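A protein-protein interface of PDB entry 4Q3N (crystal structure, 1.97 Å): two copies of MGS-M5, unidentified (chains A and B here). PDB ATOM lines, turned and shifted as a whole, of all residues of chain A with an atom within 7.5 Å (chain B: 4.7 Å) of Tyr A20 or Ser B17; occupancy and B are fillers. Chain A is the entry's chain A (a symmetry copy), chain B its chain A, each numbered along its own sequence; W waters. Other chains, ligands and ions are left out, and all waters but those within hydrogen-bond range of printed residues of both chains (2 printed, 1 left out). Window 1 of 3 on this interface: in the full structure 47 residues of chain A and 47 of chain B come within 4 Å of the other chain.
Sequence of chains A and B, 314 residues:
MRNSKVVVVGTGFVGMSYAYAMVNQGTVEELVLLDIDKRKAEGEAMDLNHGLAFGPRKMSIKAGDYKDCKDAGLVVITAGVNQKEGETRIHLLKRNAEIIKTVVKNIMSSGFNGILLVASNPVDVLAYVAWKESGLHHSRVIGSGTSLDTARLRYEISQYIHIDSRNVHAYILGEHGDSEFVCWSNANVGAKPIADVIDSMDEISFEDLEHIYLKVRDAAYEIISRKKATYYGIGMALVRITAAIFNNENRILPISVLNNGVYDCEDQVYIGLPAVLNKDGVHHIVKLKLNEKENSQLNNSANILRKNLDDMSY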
ATOM      1  N   VAL A  14     -27.973 -21.561  -2.917  1.00  0.00           N
ATOM      2  CA  VAL A  14     -29.445 -21.720  -3.071  1.00  0.00           C
ATOM      3  C   VAL A  14     -29.869 -21.660  -4.545  1.00  0.00           C
ATOM      4  O   VAL A  14     -30.529 -22.575  -5.057  1.00  0.00           O
ATOM      5  CB  VAL A  14     -30.211 -20.650  -2.238  1.00  0.00           C
ATOM      6  CG1 VAL A  14     -31.686 -20.683  -2.561  1.00  0.00           C
ATOM      7  CG2 VAL A  14     -29.994 -20.880  -0.709  1.00  0.00           C
ATOM      8  N   GLY A  15     -29.435 -20.630  -5.255  1.00  0.00           N
ATOM      9  CA  GLY A  15     -29.851 -20.491  -6.652  1.00  0.00           C
ATOM     10  C   GLY A  15     -29.332 -21.659  -7.489  1.00  0.00           C
ATOM     11  O   GLY A  15     -30.033 -22.157  -8.399  1.00  0.00           O
ATOM     12  N   MET A  16     -28.109 -22.106  -7.203  1.00  0.00           N
ATOM     13  CA  MET A  16     -27.509 -23.109  -8.079  1.00  0.00           C
ATOM     14  C   MET A  16     -28.011 -24.540  -7.721  1.00  0.00           C
ATOM     15  O   MET A  16     -28.072 -25.380  -8.588  1.00  0.00           O
ATOM     16  CB  MET A  16     -25.975 -23.060  -8.043  1.00  0.00           C
ATOM     17  CG  MET A  16     -25.413 -21.784  -8.744  1.00  0.00           C
ATOM     18  SD  MET A  16     -26.016 -21.612 -10.433  1.00  0.00           S
ATOM     19  CE  MET A  16     -25.666 -23.241 -11.199  1.00  0.00           C
ATOM     20  N   SER A  17     -28.321 -24.802  -6.464  1.00  0.00           N
ATOM     21  CA  SER A  17     -28.916 -26.089  -6.100  1.00  0.00           C
ATOM     22  C   SER A  17     -30.288 -26.190  -6.774  1.00  0.00           C
ATOM     23  O   SER A  17     -30.658 -27.206  -7.358  1.00  0.00           O
ATOM     24  CB  SER A  17     -29.022 -26.197  -4.583  1.00  0.00           C
ATOM     25  OG  SER A  17     -27.713 -26.360  -4.035  1.00  0.00           O
ATOM     26  N   TYR A  18     -31.008 -25.083  -6.763  1.00  0.00           N
ATOM     27  CA  TYR A  18     -32.269 -24.998  -7.491  1.00  0.00           C
ATOM     28  C   TYR A  18     -32.069 -25.278  -9.001  1.00  0.00           C
ATOM     29  O   TYR A  18     -32.750 -26.157  -9.594  1.00  0.00           O
ATOM     30  CB  TYR A  18     -32.878 -23.604  -7.278  1.00  0.00           C
ATOM     31  CG  TYR A  18     -34.028 -23.260  -8.231  1.00  0.00           C
ATOM     32  CD1 TYR A  18     -35.153 -24.080  -8.346  1.00  0.00           C
ATOM     33  CD2 TYR A  18     -33.986 -22.102  -8.986  1.00  0.00           C
ATOM     34  CE1 TYR A  18     -36.242 -23.732  -9.230  1.00  0.00           C
ATOM     35  CE2 TYR A  18     -35.063 -21.720  -9.846  1.00  0.00           C
ATOM     36  CZ  TYR A  18     -36.184 -22.544  -9.948  1.00  0.00           C
ATOM     37  OH  TYR A  18     -37.217 -22.182 -10.793  1.00  0.00           O
ATOM     38  N   ALA A  19     -31.134 -24.574  -9.629  1.00  0.00           N
ATOM     39  CA  ALA A  19     -30.873 -24.781 -11.041  1.00  0.00           C
ATOM     40  C   ALA A  19     -30.456 -26.250 -11.327  1.00  0.00           C
ATOM     41  O   ALA A  19     -30.984 -26.864 -12.263  1.00  0.00           O
ATOM     42  CB  ALA A  19     -29.805 -23.828 -11.537  1.00  0.00           C
ATOM     43  N   TYR A  20     -29.565 -26.803 -10.500  1.00  0.00           N
ATOM     44  CA  TYR A  20     -29.084 -28.154 -10.776  1.00  0.00           C
ATOM     45  C   TYR A  20     -30.226 -29.143 -10.619  1.00  0.00           C
ATOM     46  O   TYR A  20     -30.303 -30.132 -11.352  1.00  0.00           O
ATOM     47  CB  TYR A  20     -27.990 -28.538  -9.821  1.00  0.00           C
ATOM     48  CG  TYR A  20     -27.177 -29.790 -10.136  1.00  0.00           C
ATOM     49  CD1 TYR A  20     -26.576 -29.991 -11.398  1.00  0.00           C
ATOM     50  CD2 TYR A  20     -26.896 -30.674  -9.133  1.00  0.00           C
ATOM     51  CE1 TYR A  20     -25.732 -31.096 -11.596  1.00  0.00           C
ATOM     52  CE2 TYR A  20     -26.050 -31.769  -9.323  1.00  0.00           C
ATOM     53  CZ  TYR A  20     -25.471 -31.942 -10.544  1.00  0.00           C
ATOM     54  OH  TYR A  20     -24.622 -33.010 -10.643  1.00  0.00           O
ATOM     55  N   ALA A  21     -31.047 -28.939  -9.597  1.00  0.00           N
ATOM     56  CA  ALA A  21     -32.185 -29.842  -9.387  1.00  0.00           C
ATOM     57  C   ALA A  21     -33.123 -29.798 -10.596  1.00  0.00           C
ATOM     58  O   ALA A  21     -33.622 -30.861 -11.049  1.00  0.00           O
ATOM     59  CB  ALA A  21     -32.940 -29.488  -8.043  1.00  0.00           C
ATOM     60  N   MET A  22     -33.351 -28.595 -11.145  1.00  0.00           N
ATOM     61  CA  MET A  22     -34.171 -28.464 -12.374  1.00  0.00           C
ATOM     62  C   MET A  22     -33.579 -29.188 -13.561  1.00  0.00           C
ATOM     63  O   MET A  22     -34.319 -29.813 -14.333  1.00  0.00           O
ATOM     64  CB  MET A  22     -34.382 -26.994 -12.763  1.00  0.00           C
ATOM     65  CG  MET A  22     -35.477 -26.352 -11.859  1.00  0.00           C
ATOM     66  SD  MET A  22     -36.205 -24.946 -12.670  1.00  0.00           S
ATOM     67  CE  MET A  22     -34.794 -23.886 -12.655  1.00  0.00           C
ATOM     68  N   VAL A  23     -32.260 -29.077 -13.723  1.00  0.00           N
ATOM     69  CA  VAL A  23     -31.573 -29.805 -14.790  1.00  0.00           C
ATOM     70  C   VAL A  23     -31.754 -31.320 -14.617  1.00  0.00           C
ATOM     71  O   VAL A  23     -32.011 -32.046 -15.591  1.00  0.00           O
ATOM     72  CB  VAL A  23     -30.084 -29.471 -14.826  1.00  0.00           C
ATOM     73  CG1 VAL A  23     -29.330 -30.390 -15.818  1.00  0.00           C
ATOM     74  CG2 VAL A  23     -29.904 -28.001 -15.222  1.00  0.00           C
ATOM     75  N   ASN A  24     -31.601 -31.824 -13.402  1.00  0.00           N
ATOM     76  CA  ASN A  24     -31.753 -33.256 -13.202  1.00  0.00           C
ATOM     77  C   ASN A  24     -33.205 -33.755 -13.294  1.00  0.00           C
ATOM     78  O   ASN A  24     -33.415 -34.909 -13.569  1.00  0.00           O
ATOM     79  CB  ASN A  24     -31.169 -33.614 -11.859  1.00  0.00           C
ATOM     80  CG  ASN A  24     -29.639 -33.693 -11.939  1.00  0.00           C
ATOM     81  OD1 ASN A  24     -29.119 -34.715 -12.392  1.00  0.00           O
ATOM     82  ND2 ASN A  24     -28.927 -32.606 -11.571  1.00  0.00           N
ATOM     83  N   GLN A  25     -34.171 -32.886 -12.970  1.00  0.00           N
ATOM     84  CA  GLN A  25     -35.579 -33.237 -13.100  1.00  0.00           C
ATOM     85  C   GLN A  25     -36.113 -32.884 -14.493  1.00  0.00           C
ATOM     86  O   GLN A  25     -37.224 -33.254 -14.798  1.00  0.00           O
ATOM     87  CB  GLN A  25     -36.434 -32.528 -12.017  1.00  0.00           C
ATOM     88  CG  GLN A  25     -36.118 -33.026 -10.582  1.00  0.00           C
ATOM     89  CD  GLN A  25     -37.199 -32.596  -9.604  1.00  0.00           C
ATOM     90  OE1 GLN A  25     -38.390 -32.526  -9.979  1.00  0.00           O
ATOM     91  NE2 GLN A  25     -36.806 -32.265  -8.347  1.00  0.00           N
ATOM     92  N   GLY A  26     -35.361 -32.151 -15.311  1.00  0.00           N
ATOM     93  CA  GLY A  26     -35.927 -31.656 -16.587  1.00  0.00           C
ATOM     94  C   GLY A  26     -37.173 -30.779 -16.424  1.00  0.00           C
ATOM     95  O   GLY A  26     -38.147 -30.890 -17.169  1.00  0.00           O
ATOM     96  N   LEU A  31     -32.988 -21.942 -19.113  1.00  0.00           N
ATOM     97  CA  LEU A  31     -32.530 -21.424 -17.838  1.00  0.00           C
ATOM     98  C   LEU A  31     -31.539 -20.290 -18.105  1.00  0.00           C
ATOM     99  O   LEU A  31     -30.642 -20.465 -18.938  1.00  0.00           O
ATOM    100  CB  LEU A  31     -31.864 -22.557 -17.073  1.00  0.00           C
ATOM    101  CG  LEU A  31     -31.329 -22.417 -15.676  1.00  0.00           C
ATOM    102  CD1 LEU A  31     -32.484 -21.987 -14.814  1.00  0.00           C
ATOM    103  CD2 LEU A  31     -30.720 -23.756 -15.215  1.00  0.00           C
ATOM    104  N   LEU A  33     -28.908 -17.668 -15.981  1.00  0.00           N
ATOM    105  CA  LEU A  33     -28.300 -17.402 -14.688  1.00  0.00           C
ATOM    106  C   LEU A  33     -27.773 -15.971 -14.655  1.00  0.00           C
ATOM    107  O   LEU A  33     -27.014 -15.559 -15.564  1.00  0.00           O
ATOM    108  CB  LEU A  33     -27.138 -18.372 -14.426  1.00  0.00           C
ATOM    109  CG  LEU A  33     -27.519 -19.863 -14.592  1.00  0.00           C
ATOM    110  CD1 LEU A  33     -26.260 -20.686 -14.328  1.00  0.00           C
ATOM    111  CD2 LEU A  33     -28.641 -20.301 -13.608  1.00  0.00           C
ATOM    112  N   ASP A  47     -20.708 -25.365 -16.032  1.00  0.00           N
ATOM    113  CA  ASP A  47     -20.682 -26.576 -15.202  1.00  0.00           C
ATOM    114  C   ASP A  47     -22.028 -27.307 -15.349  1.00  0.00           C
ATOM    115  O   ASP A  47     -22.060 -28.546 -15.406  1.00  0.00           O
ATOM    116  CB  ASP A  47     -20.396 -26.212 -13.722  1.00  0.00           C
ATOM    117  CG  ASP A  47     -19.800 -27.364 -12.905  1.00  0.00           C
ATOM    118  OD1 ASP A  47     -19.324 -28.383 -13.482  1.00  0.00           O
ATOM    119  OD2 ASP A  47     -19.776 -27.225 -11.644  1.00  0.00           O
ATOM    120  N   LEU A  48     -23.127 -26.544 -15.413  1.00  0.00           N
ATOM    121  CA  LEU A  48     -24.452 -27.177 -15.650  1.00  0.00           C
ATOM    122  C   LEU A  48     -24.512 -27.770 -17.044  1.00  0.00           C
ATOM    123  O   LEU A  48     -24.956 -28.896 -17.192  1.00  0.00           O
ATOM    124  CB  LEU A  48     -25.589 -26.189 -15.491  1.00  0.00           C
ATOM    125  CG  LEU A  48     -25.925 -25.673 -14.084  1.00  0.00           C
ATOM    126  CD1 LEU A  48     -27.147 -24.711 -14.211  1.00  0.00           C
ATOM    127  CD2 LEU A  48     -26.256 -26.822 -13.132  1.00  0.00           C
ATOM    128  N   GLY A  51     -23.169 -31.318 -17.927  1.00  0.00           N
ATOM    129  CA  GLY A  51     -23.845 -32.550 -17.500  1.00  0.00           C
ATOM    130  C   GLY A  51     -25.045 -32.897 -18.413  1.00  0.00           C
ATOM    131  O   GLY A  51     -25.613 -34.000 -18.324  1.00  0.00           O
ATOM    132  N   MET A  59     -31.947 -28.926 -22.908  1.00  0.00           N
ATOM    133  CA  MET A  59     -32.124 -27.601 -22.323  1.00  0.00           C
ATOM    134  C   MET A  59     -31.210 -26.601 -22.943  1.00  0.00           C
ATOM    135  O   MET A  59     -30.188 -26.961 -23.503  1.00  0.00           O
ATOM    136  CB  MET A  59     -31.841 -27.630 -20.795  1.00  0.00           C
ATOM    137  CG  MET A  59     -32.845 -28.499 -20.041  1.00  0.00           C
ATOM    138  SD  MET A  59     -32.513 -28.564 -18.268  1.00  0.00           S
ATOM    139  CE  MET A  59     -32.832 -26.855 -17.789  1.00  0.00           C
ATOM    140  N   TYR A 232     -29.758 -27.820  -0.223  1.00  0.00           N
ATOM    141  CA  TYR A 232     -30.390 -28.877  -1.029  1.00  0.00           C
ATOM    142  C   TYR A 232     -31.909 -28.911  -0.813  1.00  0.00           C
ATOM    143  O   TYR A 232     -32.725 -29.038  -1.762  1.00  0.00           O
ATOM    144  CB  TYR A 232     -29.746 -30.241  -0.710  1.00  0.00           C
ATOM    145  CG  TYR A 232     -28.293 -30.324  -1.187  1.00  0.00           C
ATOM    146  CD1 TYR A 232     -27.949 -29.900  -2.462  1.00  0.00           C
ATOM    147  CD2 TYR A 232     -27.291 -30.824  -0.354  1.00  0.00           C
ATOM    148  CE1 TYR A 232     -26.632 -29.968  -2.910  1.00  0.00           C
ATOM    149  CE2 TYR A 232     -25.976 -30.900  -0.784  1.00  0.00           C
ATOM    150  CZ  TYR A 232     -25.656 -30.458  -2.062  1.00  0.00           C
ATOM    151  OH  TYR A 232     -24.345 -30.484  -2.484  1.00  0.00           O
ATOM    152  N   VAL A 239     -37.964 -26.066  -6.915  1.00  0.00           N
ATOM    153  CA  VAL A 239     -38.333 -26.855  -8.102  1.00  0.00           C
ATOM    154  C   VAL A 239     -39.814 -27.193  -8.074  1.00  0.00           C
ATOM    155  O   VAL A 239     -40.544 -27.064  -9.088  1.00  0.00           O
ATOM    156  CB  VAL A 239     -37.503 -28.145  -8.202  1.00  0.00           C
ATOM    157  CG1 VAL A 239     -38.099 -29.035  -9.366  1.00  0.00           C
ATOM    158  CG2 VAL A 239     -36.056 -27.748  -8.466  1.00  0.00           C
ATOM    159  N   PHE B  13     -18.058 -31.243  -2.612  1.00  0.00           N
ATOM    160  CA  PHE B  13     -19.058 -30.920  -3.610  1.00  0.00           C
ATOM    161  C   PHE B  13     -19.172 -31.973  -4.704  1.00  0.00           C
ATOM    162  O   PHE B  13     -20.233 -32.116  -5.272  1.00  0.00           O
ATOM    163  CB  PHE B  13     -18.792 -29.542  -4.219  1.00  0.00           C
ATOM    164  CG  PHE B  13     -18.970 -28.439  -3.209  1.00  0.00           C
ATOM    165  CD1 PHE B  13     -20.241 -28.080  -2.793  1.00  0.00           C
ATOM    166  CD2 PHE B  13     -17.889 -27.842  -2.610  1.00  0.00           C
ATOM    167  CE1 PHE B  13     -20.427 -27.085  -1.832  1.00  0.00           C
ATOM    168  CE2 PHE B  13     -18.065 -26.848  -1.645  1.00  0.00           C
ATOM    169  CZ  PHE B  13     -19.349 -26.496  -1.249  1.00  0.00           C
ATOM    170  N   VAL B  14     -18.118 -32.721  -5.002  1.00  0.00           N
ATOM    171  CA  VAL B  14     -18.304 -33.812  -6.000  1.00  0.00           C
ATOM    172  C   VAL B  14     -19.248 -34.903  -5.474  1.00  0.00           C
ATOM    173  O   VAL B  14     -20.252 -35.242  -6.116  1.00  0.00           O
ATOM    174  CB  VAL B  14     -16.935 -34.428  -6.414  1.00  0.00           C
ATOM    175  CG1 VAL B  14     -17.143 -35.663  -7.258  1.00  0.00           C
ATOM    176  CG2 VAL B  14     -16.074 -33.386  -7.195  1.00  0.00           C
ATOM    177  N   GLY B  15     -18.982 -35.405  -4.278  1.00  0.00           N
ATOM    178  CA  GLY B  15     -19.815 -36.485  -3.748  1.00  0.00           C
ATOM    179  C   GLY B  15     -21.254 -36.010  -3.549  1.00  0.00           C
ATOM    180  O   GLY B  15     -22.220 -36.768  -3.795  1.00  0.00           O
ATOM    181  N   MET B  16     -21.418 -34.765  -3.100  1.00  0.00           N
ATOM    182  CA  MET B  16     -22.762 -34.323  -2.741  1.00  0.00           C
ATOM    183  C   MET B  16     -23.561 -33.872  -4.001  1.00  0.00           C
ATOM    184  O   MET B  16     -24.765 -33.985  -4.011  1.00  0.00           O
ATOM    185  CB  MET B  16     -22.739 -33.199  -1.696  1.00  0.00           C
ATOM    186  CG  MET B  16     -22.289 -33.712  -0.293  1.00  0.00           C
ATOM    187  SD  MET B  16     -23.291 -35.094   0.282  1.00  0.00           S
ATOM    188  CE  MET B  16     -25.017 -34.500   0.095  1.00  0.00           C
ATOM    189  N   SER B  17     -22.895 -33.342  -5.011  1.00  0.00           N
ATOM    190  CA  SER B  17     -23.582 -33.020  -6.263  1.00  0.00           C
ATOM    191  C   SER B  17     -24.079 -34.328  -6.887  1.00  0.00           C
ATOM    192  O   SER B  17     -25.213 -34.445  -7.345  1.00  0.00           O
ATOM    193  CB  SER B  17     -22.630 -32.276  -7.194  1.00  0.00           C
ATOM    194  OG  SER B  17     -22.411 -30.961  -6.682  1.00  0.00           O
ATOM    195  N   TYR B  18     -23.240 -35.345  -6.815  1.00  0.00           N
ATOM    196  CA  TYR B  18     -23.641 -36.681  -7.240  1.00  0.00           C
ATOM    197  C   TYR B  18     -24.875 -37.180  -6.446  1.00  0.00           C
ATOM    198  O   TYR B  18     -25.906 -37.591  -7.041  1.00  0.00           O
ATOM    199  CB  TYR B  18     -22.457 -37.643  -7.054  1.00  0.00           C
ATOM    200  CG  TYR B  18     -22.822 -39.128  -7.151  1.00  0.00           C
ATOM    201  CD1 TYR B  18     -23.477 -39.649  -8.271  1.00  0.00           C
ATOM    202  CD2 TYR B  18     -22.483 -39.999  -6.132  1.00  0.00           C
ATOM    203  CE1 TYR B  18     -23.793 -41.056  -8.361  1.00  0.00           C
ATOM    204  CE2 TYR B  18     -22.758 -41.400  -6.210  1.00  0.00           C
ATOM    205  CZ  TYR B  18     -23.407 -41.910  -7.336  1.00  0.00           C
ATOM    206  OH  TYR B  18     -23.688 -43.261  -7.402  1.00  0.00           O
ATOM    207  N   ALA B  19     -24.803 -37.127  -5.121  1.00  0.00           N
ATOM    208  CA  ALA B  19     -25.918 -37.563  -4.301  1.00  0.00           C
ATOM    209  C   ALA B  19     -27.202 -36.747  -4.616  1.00  0.00           C
ATOM    210  O   ALA B  19     -28.275 -37.339  -4.791  1.00  0.00           O
ATOM    211  CB  ALA B  19     -25.579 -37.455  -2.829  1.00  0.00           C
ATOM    212  N   TYR B  20     -27.070 -35.423  -4.734  1.00  0.00           N
ATOM    213  CA  TYR B  20     -28.262 -34.608  -4.951  1.00  0.00           C
ATOM    214  C   TYR B  20     -28.856 -34.927  -6.312  1.00  0.00           C
ATOM    215  O   TYR B  20     -30.078 -34.917  -6.480  1.00  0.00           O
ATOM    216  CB  TYR B  20     -27.924 -33.145  -4.912  1.00  0.00           C
ATOM    217  CG  TYR B  20     -29.077 -32.150  -4.834  1.00  0.00           C
ATOM    218  CD1 TYR B  20     -30.094 -32.261  -3.860  1.00  0.00           C
ATOM    219  CD2 TYR B  20     -29.055 -31.037  -5.626  1.00  0.00           C
ATOM    220  CE1 TYR B  20     -31.061 -31.249  -3.746  1.00  0.00           C
ATOM    221  CE2 TYR B  20     -30.009 -30.024  -5.511  1.00  0.00           C
ATOM    222  CZ  TYR B  20     -30.977 -30.144  -4.559  1.00  0.00           C
ATOM    223  OH  TYR B  20     -31.850 -29.093  -4.477  1.00  0.00           O
ATOM    224  N   ALA B  21     -27.994 -35.100  -7.305  1.00  0.00           N
ATOM    225  CA  ALA B  21     -28.489 -35.427  -8.649  1.00  0.00           C
ATOM    226  C   ALA B  21     -29.253 -36.753  -8.620  1.00  0.00           C
ATOM    227  O   ALA B  21     -30.331 -36.878  -9.260  1.00  0.00           O
ATOM    228  CB  ALA B  21     -27.301 -35.455  -9.692  1.00  0.00           C
ATOM    229  N   TYR B 231     -18.100 -29.305 -10.303  1.00  0.00           N
ATOM    230  CA  TYR B 231     -18.758 -30.438  -9.653  1.00  0.00           C
ATOM    231  C   TYR B 231     -20.136 -30.797 -10.204  1.00  0.00           C
ATOM    232  O   TYR B 231     -20.541 -31.934 -10.066  1.00  0.00           O
ATOM    233  CB  TYR B 231     -18.893 -30.220  -8.128  1.00  0.00           C
ATOM    234  CG  TYR B 231     -19.246 -28.806  -7.674  1.00  0.00           C
ATOM    235  CD1 TYR B 231     -20.563 -28.392  -7.550  1.00  0.00           C
ATOM    236  CD2 TYR B 231     -18.213 -27.882  -7.320  1.00  0.00           C
ATOM    237  CE1 TYR B 231     -20.873 -27.079  -7.078  1.00  0.00           C
ATOM    238  CE2 TYR B 231     -18.506 -26.589  -6.945  1.00  0.00           C
ATOM    239  CZ  TYR B 231     -19.832 -26.204  -6.810  1.00  0.00           C
ATOM    240  OH  TYR B 231     -20.081 -24.933  -6.386  1.00  0.00           O
ATOM    241  N   TYR B 232     -20.855 -29.869 -10.834  1.00  0.00           N
ATOM    242  CA  TYR B 232     -22.163 -30.274 -11.373  1.00  0.00           C
ATOM    243  C   TYR B 232     -22.005 -31.265 -12.534  1.00  0.00           C
ATOM    244  O   TYR B 232     -22.722 -32.293 -12.647  1.00  0.00           O
ATOM    245  CB  TYR B 232     -22.965 -29.029 -11.802  1.00  0.00           C
ATOM    246  CG  TYR B 232     -23.384 -28.167 -10.608  1.00  0.00           C
ATOM    247  CD1 TYR B 232     -23.944 -28.754  -9.481  1.00  0.00           C
ATOM    248  CD2 TYR B 232     -23.211 -26.782 -10.626  1.00  0.00           C
ATOM    249  CE1 TYR B 232     -24.328 -27.984  -8.387  1.00  0.00           C
ATOM    250  CE2 TYR B 232     -23.590 -26.001  -9.546  1.00  0.00           C
ATOM    251  CZ  TYR B 232     -24.137 -26.615  -8.426  1.00  0.00           C
ATOM    252  OH  TYR B 232     -24.474 -25.854  -7.328  1.00  0.00           O
ATOM    253  N   GLY B 235     -20.973 -34.705 -11.287  1.00  0.00           N
ATOM    254  CA  GLY B 235     -22.095 -35.282 -10.559  1.00  0.00           C
ATOM    255  C   GLY B 235     -23.057 -36.026 -11.490  1.00  0.00           C
ATOM    256  O   GLY B 235     -23.505 -37.143 -11.192  1.00  0.00           O
ATOM    257  N   MET B 236     -23.396 -35.421 -12.617  1.00  0.00           N
ATOM    258  CA  MET B 236     -24.336 -36.083 -13.561  1.00  0.00           C
ATOM    259  C   MET B 236     -23.681 -37.239 -14.337  1.00  0.00           C
ATOM    260  O   MET B 236     -24.354 -38.216 -14.703  1.00  0.00           O
ATOM    261  CB  MET B 236     -24.899 -35.033 -14.524  1.00  0.00           C
ATOM    262  CG  MET B 236     -25.902 -34.096 -13.766  1.00  0.00           C
ATOM    263  SD  MET B 236     -26.719 -32.899 -14.815  1.00  0.00           S
ATOM    264  CE  MET B 236     -27.887 -34.018 -15.701  1.00  0.00           C
HETATM  265  O   HOH W   1     -25.466 -27.247  -5.228  1.00  0.00           O
HETATM  266  O   HOH W   2     -23.924 -29.521  -4.980  1.00  0.00           O
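OH of Tyr B20 sits at hydrogen-bond distance from O of Tyr A232, at 2.9 Å. N of Tyr B232 sits at hydrogen-bond distance from OD2 of Asp A47 (3.0 Å). The backbone NH (N) of Met B236 lies within hydrogen-bond range of the side-chain hydroxyl (OH) of Tyr A20 (3.3 Å). The backbone NH (N) of Tyr B231 lies within hydrogen-bond range of the side-chain carboxylate (OD2) of Asp A47 (3.0 Å). The side-chain hydroxyl (OH) of Tyr A20 lies within hydrogen-bond range of the backbone carbonyl oxygen (O) of Tyr B232 (2.9 Å).
The backbone carbonyl oxygen (O) of Tyr A20 lies within hydrogen-bond range of the side-chain amide nitrogen (ND2) of Asn A24 (2.8 Å). OG of Ser B17 lies within hydrogen-bond range of O of Phe B13, 2.8 Å away.
Tyr B20 touches Ser A17 (CE2 to O, 3.4 Å). Tyr A20 touches Ser B17. Tyr A20 touches Ala B21. Ala A21 touches Tyr B20 (CB to OH, 3.7 Å). Met B236 touches Val A23 (SD to CG1, 3.8 Å). OD1 of Asn A24 touches CB of Ala B21, at 3.3 Å. Asn A24 touches Met B236. CD2 of Leu A48 touches CD2 of Tyr B232, 3.9 Å away. O of Gly A51 touches CE of Met B236, 3.5 Å away. OH of Tyr A232 touches CB of Met B16 (3.3 Å).
Tyr A20 touches just these residues of chain B: Ser B17 (3.4 Å), Ala B21 (3.7 Å), Tyr B232 (2.9 Å), Gly B235 (3.4 Å) and Met B236 (3.3 Å). Ser B17 touches just one residue of chain A: Tyr A20 (3.4 Å). Printed residues of chain B within 4 Å of Met A16: Tyr B232. Of the printed residues of chain A, Met B16 touches Tyr A232 (3.3 Å). Of the printed residues of chain A, Met B236 touches Tyr A20, Val A23, Asn A24 and Gly A51. Tyr B18 touches none of the printed residues of chain A. Tyr A18 touches none of the printed residues of chain B. The nearest residue of chain B that does not touch Tyr A20 is Tyr B20 (4.1 Å). The nearest residue of chain A that does not touch Ser B17 is Tyr A232 (4.1 Å). The nearest printed residue of chain B that does not touch Gly A51 is Tyr B232 (5.0 Å).
Of the 13 printed residues of chain B, 8 touch a printed residue of chain A. Hydrophobic or aromatic side chains of chain A that line the printed part of chain B: Met A16, Tyr A20, Ala A21, Val A23, Leu A48 and Tyr A232.
Met A16 touches Tyr B232, and with the chains exchanged Tyr A232 touches Met B16. Ser A17 touches Tyr B20, and with the chains exchanged Tyr A20 touches Ser B17. Tyr A20 touches Ala B21, and with the chains exchanged Ala A21 touches Tyr B20. Tyr A20 touches Tyr B232, and with the chains exchanged Tyr A232 touches Tyr B20. Of the 17 pairs that touch across the chains among the printed residues, 8 have their exchanged pair printed and touching as well.
Water W2 bridges OG of Ser B17 (2.7 Å) and OH of Tyr A232 (2.7 Å). Water W1 bridges OG of Ser A17 (2.7 Å) and OH of Tyr B232 (2.7 Å).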
